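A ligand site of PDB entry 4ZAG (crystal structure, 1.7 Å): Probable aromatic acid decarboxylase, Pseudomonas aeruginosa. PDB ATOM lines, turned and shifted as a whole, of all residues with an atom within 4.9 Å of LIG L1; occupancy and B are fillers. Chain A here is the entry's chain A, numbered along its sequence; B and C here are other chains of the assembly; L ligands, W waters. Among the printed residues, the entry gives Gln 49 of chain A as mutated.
NH2 of Arg 139 is in salt-bridge range of O3 of LG2 L2 (3.2 Å).
O9 of LIG L1 lies within hydrogen-bond range of OG of Ser 104 (2.5 Å).
O9 of LIG L1 sits at hydrogen-bond distance from OG1 of Thr 107 (2.7 Å).
The side-chain hydroxyl (OG1) of Thr 105 sits at hydrogen-bond distance from an oxygen (O1) of LIG L1 (3.4 Å).
O8 of LIG L1 lies within hydrogen-bond range of OG of Ser 39, 2.6 Å away.
An oxygen (O5) of LIG L1 is in hydrogen-bond range of the backbone carbonyl oxygen (O) of Cys 116 of chain B (2.8 Å).
N of Thr 105 lies within hydrogen-bond range of O1 of LIG L1.
O of Gly 13 sits at hydrogen-bond distance from O3 of LIG L1.
O of Arg 139 is in hydrogen-bond range of N2 of LIG L1 (3.1 Å).
An oxygen (O8) of LIG L1 lies within hydrogen-bond range of the backbone NH of Gly 13 (2.7 Å).
O3 of LG2 L2 lies within hydrogen-bond range of OH of Tyr 169 of chain C, at 3.0 Å.
An oxygen (O2) of LG2 L2 sits close to the side-chain carboxylate (OE1) of Glu 140, at 2.4 Å.
The backbone NH (N) of Ser 15 is in hydrogen-bond range of an oxygen (O2) of LIG L1, at 3.0 Å.
The guanidinium group of Arg 122 of chain B lies within salt-bridge range of an oxygen (O2) of LG2 L2 (2.9 Å).
The guanidinium group (NH2) of Arg 139 lies within hydrogen-bond range of an oxygen (O2) of LIG L1, at 2.7 Å.
The backbone carbonyl oxygen of Trp 84 of chain B is in hydrogen-bond range of the indole nitrogen of Trp 200 of chain C, at 2.9 Å.
The side-chain hydroxyl (OG1) of Thr 105 is in hydrogen-bond range of the guanidinium group (NH1) of Arg 122 of chain B, at 3.4 Å.
OG of Ser 39 sits at hydrogen-bond distance from N of Ala 42.
OE2 of Glu 140 lies within salt-bridge range of NH1 of Arg 122 of chain B (2.9 Å).
The side-chain hydroxyl (OG) of Ser 39 lies close to the backbone NH (N) of Ala 41.
The backbone NH (N) of Ser 104 sits at hydrogen-bond distance from the side-chain hydroxyl (OG1) of Thr 12, 2.9 Å away.
The side-chain amide oxygen (OE1) of Gln 49 is in hydrogen-bond range of the side-chain hydroxyl (OG1) of Thr 48, 2.9 Å away.
The side-chain hydroxyl of Ser 104 lies within hydrogen-bond range of the backbone NH of Thr 107.
O1 of LIG L1 lies close to OE2 of Glu 140, at 3.5 Å.
Merely in contact with LIG L1: Thr 12, Ala 14, Ala 41, Val 45, Gln 49, Trp 84 of chain B and Arg 122 of chain B.
Within 4 Å of LIG L1: Thr 12, Gly 13, Ala 14, Ser 15, Ser 39, Ala 41, Val 45, Gln 49, Ser 104, Thr 105, Thr 107, Arg 139, Glu 140, Trp 84 of chain B, Cys 116 of chain B and Arg 122 of chain B.
The nearest printed residue that does not touch LIG L1 is Ala 42 (4.2 Å).
Water W1 lies within hydrogen-bond range of an oxygen (O9) of LIG L1 and the backbone carbonyl oxygen of Cys 116 of chain B.
Water W2 lies within hydrogen-bond range of an oxygen (O7) of LIG L1 (2.8 Å) and the backbone NH (N) of Ala 41 (3.0 Å).
Water W3 lies within hydrogen-bond range of O4 of LIG L1 (2.8 Å), OG1 of Thr 105 (3.0 Å), N of Gly 106 (3.1 Å) and SG of Cys 116 of chain B (3.7 Å).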
ATOM      1  N   THR A  12     -30.619 -13.424   4.625  1.00  0.00           N
ATOM      2  CA  THR A  12     -29.471 -12.769   4.035  1.00  0.00           C
ATOM      3  C   THR A  12     -28.142 -13.200   4.670  1.00  0.00           C
ATOM      4  O   THR A  12     -28.115 -13.994   5.608  1.00  0.00           O
ATOM      5  CB  THR A  12     -29.622 -11.182   4.054  1.00  0.00           C
ATOM      6  OG1 THR A  12     -29.580 -10.739   5.418  1.00  0.00           O
ATOM      7  CG2 THR A  12     -30.921 -10.810   3.410  1.00  0.00           C
ATOM      8  N   GLY A  13     -27.079 -12.769   4.050  1.00  0.00           N
ATOM      9  CA  GLY A  13     -25.765 -13.296   4.247  1.00  0.00           C
ATOM     10  C   GLY A  13     -25.006 -13.004   5.503  1.00  0.00           C
ATOM     11  O   GLY A  13     -23.808 -12.811   5.418  1.00  0.00           O
ATOM     12  N   ALA A  14     -25.683 -12.932   6.622  1.00  0.00           N
ATOM     13  CA  ALA A  14     -24.996 -12.859   7.862  1.00  0.00           C
ATOM     14  C   ALA A  14     -24.827 -14.296   8.343  1.00  0.00           C
ATOM     15  O   ALA A  14     -25.609 -15.201   8.039  1.00  0.00           O
ATOM     16  CB  ALA A  14     -25.804 -12.106   8.877  1.00  0.00           C
ATOM     17  N   SER A  15     -23.875 -14.438   9.222  1.00  0.00           N
ATOM     18  CA  SER A  15     -23.672 -15.670   9.993  1.00  0.00           C
ATOM     19  C   SER A  15     -24.921 -15.883  10.820  1.00  0.00           C
ATOM     20  O   SER A  15     -25.561 -14.917  11.312  1.00  0.00           O
ATOM     21  CB  SER A  15     -22.394 -15.592  10.799  1.00  0.00           C
ATOM     22  OG  SER A  15     -22.096 -16.929  11.271  1.00  0.00           O
ATOM     23  N   SER A  39     -30.948 -14.517  -0.287  1.00  0.00           N
ATOM     24  CA  SER A  39     -29.957 -13.897  -1.098  1.00  0.00           C
ATOM     25  C   SER A  39     -28.863 -14.841  -1.562  1.00  0.00           C
ATOM     26  O   SER A  39     -28.663 -15.870  -0.965  1.00  0.00           O
ATOM     27  CB  SER A  39     -29.281 -12.727  -0.303  1.00  0.00           C
ATOM     28  OG  SER A  39     -28.373 -13.203   0.641  1.00  0.00           O
ATOM     29  N   ALA A  41     -25.637 -14.315  -1.222  1.00  0.00           N
ATOM     30  CA  ALA A  41     -24.677 -14.485  -0.120  1.00  0.00           C
ATOM     31  C   ALA A  41     -25.201 -15.415   0.968  1.00  0.00           C
ATOM     32  O   ALA A  41     -24.457 -16.203   1.539  1.00  0.00           O
ATOM     33  CB  ALA A  41     -24.259 -13.116   0.469  1.00  0.00           C
ATOM     34  N   ALA A  42     -26.501 -15.399   1.311  1.00  0.00           N
ATOM     35  CA  ALA A  42     -27.018 -16.305   2.302  1.00  0.00           C
ATOM     36  C   ALA A  42     -26.938 -17.796   1.763  1.00  0.00           C
ATOM     37  O   ALA A  42     -26.718 -18.696   2.590  1.00  0.00           O
ATOM     38  CB  ALA A  42     -28.430 -15.982   2.617  1.00  0.00           C
ATOM     39  N   VAL A  45     -23.464 -18.691   2.551  1.00  0.00           N
ATOM     40  CA  VAL A  45     -23.353 -18.970   3.963  1.00  0.00           C
ATOM     41  C   VAL A  45     -23.890 -20.397   4.341  1.00  0.00           C
ATOM     42  O   VAL A  45     -23.303 -21.150   5.111  1.00  0.00           O
ATOM     43  CB  VAL A  45     -24.071 -17.882   4.831  1.00  0.00           C
ATOM     44  CG1 VAL A  45     -24.186 -18.324   6.265  1.00  0.00           C
ATOM     45  CG2 VAL A  45     -23.336 -16.536   4.620  1.00  0.00           C
ATOM     46  N   THR A  48     -21.523 -23.173   2.673  1.00  0.00           N
ATOM     47  CA  THR A  48     -20.174 -23.285   3.187  1.00  0.00           C
ATOM     48  C   THR A  48     -20.117 -23.465   4.672  1.00  0.00           C
ATOM     49  O   THR A  48     -19.121 -23.916   5.142  1.00  0.00           O
ATOM     50  CB  THR A  48     -19.303 -22.110   2.786  1.00  0.00           C
ATOM     51  OG1 THR A  48     -19.848 -20.905   3.378  1.00  0.00           O
ATOM     52  CG2 THR A  48     -19.161 -22.035   1.241  1.00  0.00           C
ATOM     53  N   GLN A  49     -21.174 -23.243   5.420  1.00  0.00           N
ATOM     54  CA  GLN A  49     -21.141 -23.309   6.875  1.00  0.00           C
ATOM     55  C   GLN A  49     -22.236 -24.096   7.543  1.00  0.00           C
ATOM     56  O   GLN A  49     -22.354 -24.095   8.766  1.00  0.00           O
ATOM     57  CB  GLN A  49     -21.176 -21.855   7.510  1.00  0.00           C
ATOM     58  CG  GLN A  49     -20.404 -20.761   6.712  1.00  0.00           C
ATOM     59  CD  GLN A  49     -18.861 -20.820   6.705  1.00  0.00           C
ATOM     60  OE1 GLN A  49     -18.217 -20.365   5.733  1.00  0.00           O
ATOM     61  NE2 GLN A  49     -18.266 -21.341   7.764  1.00  0.00           N
ATOM     62  N   SER A 104     -27.956  -9.243   7.289  1.00  0.00           N
ATOM     63  CA  SER A 104     -26.589  -8.726   7.100  1.00  0.00           C
ATOM     64  C   SER A 104     -26.612  -7.172   7.278  1.00  0.00           C
ATOM     65  O   SER A 104     -27.650  -6.520   7.193  1.00  0.00           O
ATOM     66  CB  SER A 104     -26.140  -8.951   5.682  1.00  0.00           C
ATOM     67  OG  SER A 104     -26.875  -8.247   4.716  1.00  0.00           O
ATOM     68  N   THR A 105     -25.443  -6.624   7.559  1.00  0.00           N
ATOM     69  CA  THR A 105     -25.331  -5.180   7.652  1.00  0.00           C
ATOM     70  C   THR A 105     -25.637  -4.546   6.312  1.00  0.00           C
ATOM     71  O   THR A 105     -26.208  -3.421   6.291  1.00  0.00           O
ATOM     72  CB  THR A 105     -23.974  -4.717   8.207  1.00  0.00           C
ATOM     73  OG1 THR A 105     -22.913  -5.107   7.331  1.00  0.00           O
ATOM     74  CG2 THR A 105     -23.714  -5.197   9.580  1.00  0.00           C
ATOM     75  N   GLY A 106     -25.354  -5.199   5.154  1.00  0.00           N
ATOM     76  CA  GLY A 106     -25.697  -4.586   3.895  1.00  0.00           C
ATOM     77  C   GLY A 106     -27.160  -4.546   3.630  1.00  0.00           C
ATOM     78  O   GLY A 106     -27.638  -3.554   3.114  1.00  0.00           O
ATOM     79  N   THR A 107     -27.914  -5.565   4.055  1.00  0.00           N
ATOM     80  CA  THR A 107     -29.348  -5.562   3.901  1.00  0.00           C
ATOM     81  C   THR A 107     -30.002  -4.552   4.902  1.00  0.00           C
ATOM     82  O   THR A 107     -30.902  -3.789   4.534  1.00  0.00           O
ATOM     83  CB  THR A 107     -29.929  -6.991   3.987  1.00  0.00           C
ATOM     84  OG1 THR A 107     -29.604  -7.669   2.772  1.00  0.00           O
ATOM     85  CG2 THR A 107     -31.425  -6.881   4.061  1.00  0.00           C
ATOM     86  N   ARG A 139     -26.853  -9.870  12.828  1.00  0.00           N
ATOM     87  CA  ARG A 139     -25.806 -10.696  13.499  1.00  0.00           C
ATOM     88  C   ARG A 139     -24.426 -10.163  13.114  1.00  0.00           C
ATOM     89  O   ARG A 139     -23.855 -10.500  12.092  1.00  0.00           O
ATOM     90  CB  ARG A 139     -25.936 -12.166  13.071  1.00  0.00           C
ATOM     91  CG  ARG A 139     -25.037 -13.160  13.792  1.00  0.00           C
ATOM     92  CD  ARG A 139     -23.599 -13.142  13.302  1.00  0.00           C
ATOM     93  NE  ARG A 139     -22.689 -12.606  14.315  1.00  0.00           N
ATOM     94  CZ  ARG A 139     -21.504 -12.086  14.011  1.00  0.00           C
ATOM     95  NH1 ARG A 139     -20.719 -11.653  14.962  1.00  0.00           N
ATOM     96  NH2 ARG A 139     -21.166 -12.013  12.733  1.00  0.00           N
ATOM     97  N   GLU A 140     -23.910  -9.253  13.916  1.00  0.00           N
ATOM     98  CA  GLU A 140     -22.652  -8.564  13.630  1.00  0.00           C
ATOM     99  C   GLU A 140     -22.083  -8.188  14.987  1.00  0.00           C
ATOM    100  O   GLU A 140     -22.770  -8.017  15.986  1.00  0.00           O
ATOM    101  CB  GLU A 140     -22.905  -7.300  12.742  1.00  0.00           C
ATOM    102  CG  GLU A 140     -21.622  -6.540  12.273  1.00  0.00           C
ATOM    103  CD  GLU A 140     -20.684  -7.418  11.527  1.00  0.00           C
ATOM    104  OE1 GLU A 140     -19.933  -8.191  12.225  1.00  0.00           O
ATOM    105  OE2 GLU A 140     -20.635  -7.381  10.284  1.00  0.00           O
ATOM    106  N   TRP B  84     -15.882 -13.559  -0.581  1.00  0.00           N
ATOM    107  CA  TRP B  84     -16.088 -13.420   0.842  1.00  0.00           C
ATOM    108  C   TRP B  84     -15.143 -14.283   1.671  1.00  0.00           C
ATOM    109  O   TRP B  84     -15.019 -14.085   2.876  1.00  0.00           O
ATOM    110  CB  TRP B  84     -17.510 -13.740   1.251  1.00  0.00           C
ATOM    111  CG  TRP B  84     -18.549 -13.055   0.425  1.00  0.00           C
ATOM    112  CD1 TRP B  84     -19.453 -13.679  -0.414  1.00  0.00           C
ATOM    113  CD2 TRP B  84     -18.749 -11.633   0.211  1.00  0.00           C
ATOM    114  NE1 TRP B  84     -20.185 -12.749  -1.110  1.00  0.00           N
ATOM    115  CE2 TRP B  84     -19.791 -11.488  -0.741  1.00  0.00           C
ATOM    116  CE3 TRP B  84     -18.125 -10.465   0.722  1.00  0.00           C
ATOM    117  CZ2 TRP B  84     -20.241 -10.233  -1.202  1.00  0.00           C
ATOM    118  CZ3 TRP B  84     -18.620  -9.202   0.285  1.00  0.00           C
ATOM    119  CH2 TRP B  84     -19.633  -9.103  -0.664  1.00  0.00           C
ATOM    120  N   CYS B 116     -23.450  -2.911   1.218  1.00  0.00           N
ATOM    121  CA  CYS B 116     -22.303  -3.891   1.118  1.00  0.00           C
ATOM    122  C   CYS B 116     -22.547  -4.716  -0.148  1.00  0.00           C
ATOM    123  O   CYS B 116     -22.836  -5.899  -0.084  1.00  0.00           O
ATOM    124  CB  CYS B 116     -22.235  -4.766   2.405  1.00  0.00           C
ATOM    125  SG  CYS B 116     -21.487  -4.220   3.974  1.00  0.00           S
ATOM    126  N   ASN B 117     -22.363  -4.149  -1.310  1.00  0.00           N
ATOM    127  CA  ASN B 117     -22.744  -4.850  -2.522  1.00  0.00           C
ATOM    128  C   ASN B 117     -21.619  -5.568  -3.226  1.00  0.00           C
ATOM    129  O   ASN B 117     -21.840  -6.149  -4.260  1.00  0.00           O
ATOM    130  CB  ASN B 117     -23.482  -3.906  -3.467  1.00  0.00           C
ATOM    131  CG  ASN B 117     -24.937  -3.598  -2.929  1.00  0.00           C
ATOM    132  OD1 ASN B 117     -25.609  -4.494  -2.354  1.00  0.00           O
ATOM    133  ND2 ASN B 117     -25.376  -2.328  -3.046  1.00  0.00           N
ATOM    134  N   ARG B 122     -17.900  -4.085   1.566  1.00  0.00           N
ATOM    135  CA  ARG B 122     -17.823  -4.817   2.784  1.00  0.00           C
ATOM    136  C   ARG B 122     -16.530  -4.592   3.543  1.00  0.00           C
ATOM    137  O   ARG B 122     -16.528  -4.499   4.780  1.00  0.00           O
ATOM    138  CB  ARG B 122     -18.001  -6.339   2.499  1.00  0.00           C
ATOM    139  CG  ARG B 122     -17.864  -7.233   3.744  1.00  0.00           C
ATOM    140  CD  ARG B 122     -18.798  -6.940   4.870  1.00  0.00           C
ATOM    141  NE  ARG B 122     -18.540  -7.915   5.922  1.00  0.00           N
ATOM    142  CZ  ARG B 122     -19.078  -7.878   7.123  1.00  0.00           C
ATOM    143  NH1 ARG B 122     -20.042  -6.985   7.432  1.00  0.00           N
ATOM    144  NH2 ARG B 122     -18.678  -8.807   8.033  1.00  0.00           N
ATOM    145  N   TYR C 169     -19.402 -19.245  11.907  1.00  0.00           N
ATOM    146  CA  TYR C 169     -18.502 -19.600  10.804  1.00  0.00           C
ATOM    147  C   TYR C 169     -17.264 -20.436  11.225  1.00  0.00           C
ATOM    148  O   TYR C 169     -16.464 -20.812  10.356  1.00  0.00           O
ATOM    149  CB  TYR C 169     -18.137 -18.361   9.951  1.00  0.00           C
ATOM    150  CG  TYR C 169     -17.608 -17.151  10.699  1.00  0.00           C
ATOM    151  CD1 TYR C 169     -16.252 -17.028  11.035  1.00  0.00           C
ATOM    152  CD2 TYR C 169     -18.482 -16.065  11.031  1.00  0.00           C
ATOM    153  CE1 TYR C 169     -15.770 -15.900  11.658  1.00  0.00           C
ATOM    154  CE2 TYR C 169     -17.989 -14.920  11.681  1.00  0.00           C
ATOM    155  CZ  TYR C 169     -16.638 -14.839  11.965  1.00  0.00           C
ATOM    156  OH  TYR C 169     -16.129 -13.741  12.574  1.00  0.00           O
ATOM    157  N   TRP C 200      -9.582 -14.912   9.795  1.00  0.00           N
ATOM    158  CA  TRP C 200     -10.277 -15.202   8.551  1.00  0.00           C
ATOM    159  C   TRP C 200      -9.441 -15.018   7.303  1.00  0.00           C
ATOM    160  O   TRP C 200      -8.896 -13.961   7.079  1.00  0.00           O
ATOM    161  CB  TRP C 200     -11.534 -14.275   8.407  1.00  0.00           C
ATOM    162  CG  TRP C 200     -12.397 -14.621   7.276  1.00  0.00           C
ATOM    163  CD1 TRP C 200     -12.519 -13.928   6.098  1.00  0.00           C
ATOM    164  CD2 TRP C 200     -13.280 -15.762   7.167  1.00  0.00           C
ATOM    165  NE1 TRP C 200     -13.414 -14.570   5.270  1.00  0.00           N
ATOM    166  CE2 TRP C 200     -13.904 -15.682   5.918  1.00  0.00           C
ATOM    167  CE3 TRP C 200     -13.600 -16.836   8.037  1.00  0.00           C
ATOM    168  CZ2 TRP C 200     -14.814 -16.654   5.474  1.00  0.00           C
ATOM    169  CZ3 TRP C 200     -14.502 -17.772   7.615  1.00  0.00           C
ATOM    170  CH2 TRP C 200     -15.104 -17.693   6.347  1.00  0.00           C
HETATM  171  N1  LIG L   1     -22.156  -9.987   6.943  1.00  0.00           N
HETATM  172  C1  LIG L   1     -22.675  -9.570   8.127  1.00  0.00           C
HETATM  173  O1  LIG L   1     -23.194  -8.419   8.147  1.00  0.00           O
HETATM  174  N2  LIG L   1     -22.660 -10.298   9.261  1.00  0.00           N
HETATM  175  C2  LIG L   1     -22.120 -11.580   9.236  1.00  0.00           C
HETATM  176  O2  LIG L   1     -22.158 -12.256  10.249  1.00  0.00           O
HETATM  177  C3  LIG L   1     -21.594 -12.027   8.001  1.00  0.00           C
HETATM  178  N3  LIG L   1     -21.114 -13.332   7.954  1.00  0.00           N
HETATM  179  C4  LIG L   1     -20.712 -13.723   6.729  1.00  0.00           C
HETATM  180  C5  LIG L   1     -20.254 -15.089   6.764  1.00  0.00           C
HETATM  181  C6  LIG L   1     -19.821 -15.643   5.577  1.00  0.00           C
HETATM  182  C7  LIG L   1     -19.299 -17.046   5.580  1.00  0.00           C
HETATM  183  C8  LIG L   1     -19.850 -14.918   4.442  1.00  0.00           C
HETATM  184  C9  LIG L   1     -19.334 -15.493   3.244  1.00  0.00           C
HETATM  185  C10 LIG L   1     -20.285 -13.560   4.403  1.00  0.00           C
HETATM  186  C11 LIG L   1     -20.674 -12.968   5.593  1.00  0.00           C
HETATM  187  N4  LIG L   1     -21.113 -11.653   5.655  1.00  0.00           N
HETATM  188  C12 LIG L   1     -21.595 -11.249   6.851  1.00  0.00           C
HETATM  189  C13 LIG L   1     -21.056 -10.871   4.481  1.00  0.00           C
HETATM  190  C14 LIG L   1     -22.161 -10.642   3.531  1.00  0.00           C
HETATM  191  O3  LIG L   1     -22.610 -11.920   3.175  1.00  0.00           O
HETATM  192  C15 LIG L   1     -21.915  -9.603   2.532  1.00  0.00           C
HETATM  193  O4  LIG L   1     -21.627  -8.300   3.038  1.00  0.00           O
HETATM  194  C16 LIG L   1     -23.026  -9.672   1.478  1.00  0.00           C
HETATM  195  O5  LIG L   1     -22.814  -8.625   0.547  1.00  0.00           O
HETATM  196  C17 LIG L   1     -24.376  -9.594   2.079  1.00  0.00           C
HETATM  197  O6  LIG L   1     -25.232  -9.634   0.980  1.00  0.00           O
HETATM  198  P1  LIG L   1     -26.788  -9.842   1.265  1.00  0.00           P
HETATM  199  O7  LIG L   1     -27.489  -9.646  -0.118  1.00  0.00           O
HETATM  200  O8  LIG L   1     -27.110 -11.232   1.839  1.00  0.00           O
HETATM  201  O9  LIG L   1     -27.186  -8.737   2.297  1.00  0.00           O
HETATM  202  O1  LG2 L   2     -16.500  -9.563  11.410  1.00  0.00           O
HETATM  203  P1  LG2 L   2     -17.582 -10.578  11.148  1.00  0.00           P
HETATM  204  O2  LG2 L   2     -18.974  -9.866  10.739  1.00  0.00           O
HETATM  205  O3  LG2 L   2     -18.021 -11.499  12.212  1.00  0.00           O
HETATM  206  O4  LG2 L   2     -17.193 -11.311   9.810  1.00  0.00           O
HETATM  207  C1  LG2 L   2     -18.185 -12.280   9.287  1.00  0.00           C
HETATM  208  C2  LG2 L   2     -17.792 -12.276   7.817  1.00  0.00           C
HETATM  209  C3  LG2 L   2     -17.107 -13.397   7.183  1.00  0.00           C
HETATM  210  C4  LG2 L   2     -16.840 -14.654   8.041  1.00  0.00           C
HETATM  211  C5  LG2 L   2     -16.850 -13.382   5.664  1.00  0.00           C
HETATM  212  O   HOH W   1     -26.002  -6.489   1.184  1.00  0.00           O
HETATM  213  O   HOH W   2     -26.349 -11.517  -1.909  1.00  0.00           O
HETATM  214  O   HOH W   3     -23.011  -7.289   5.312  1.00  0.00           O
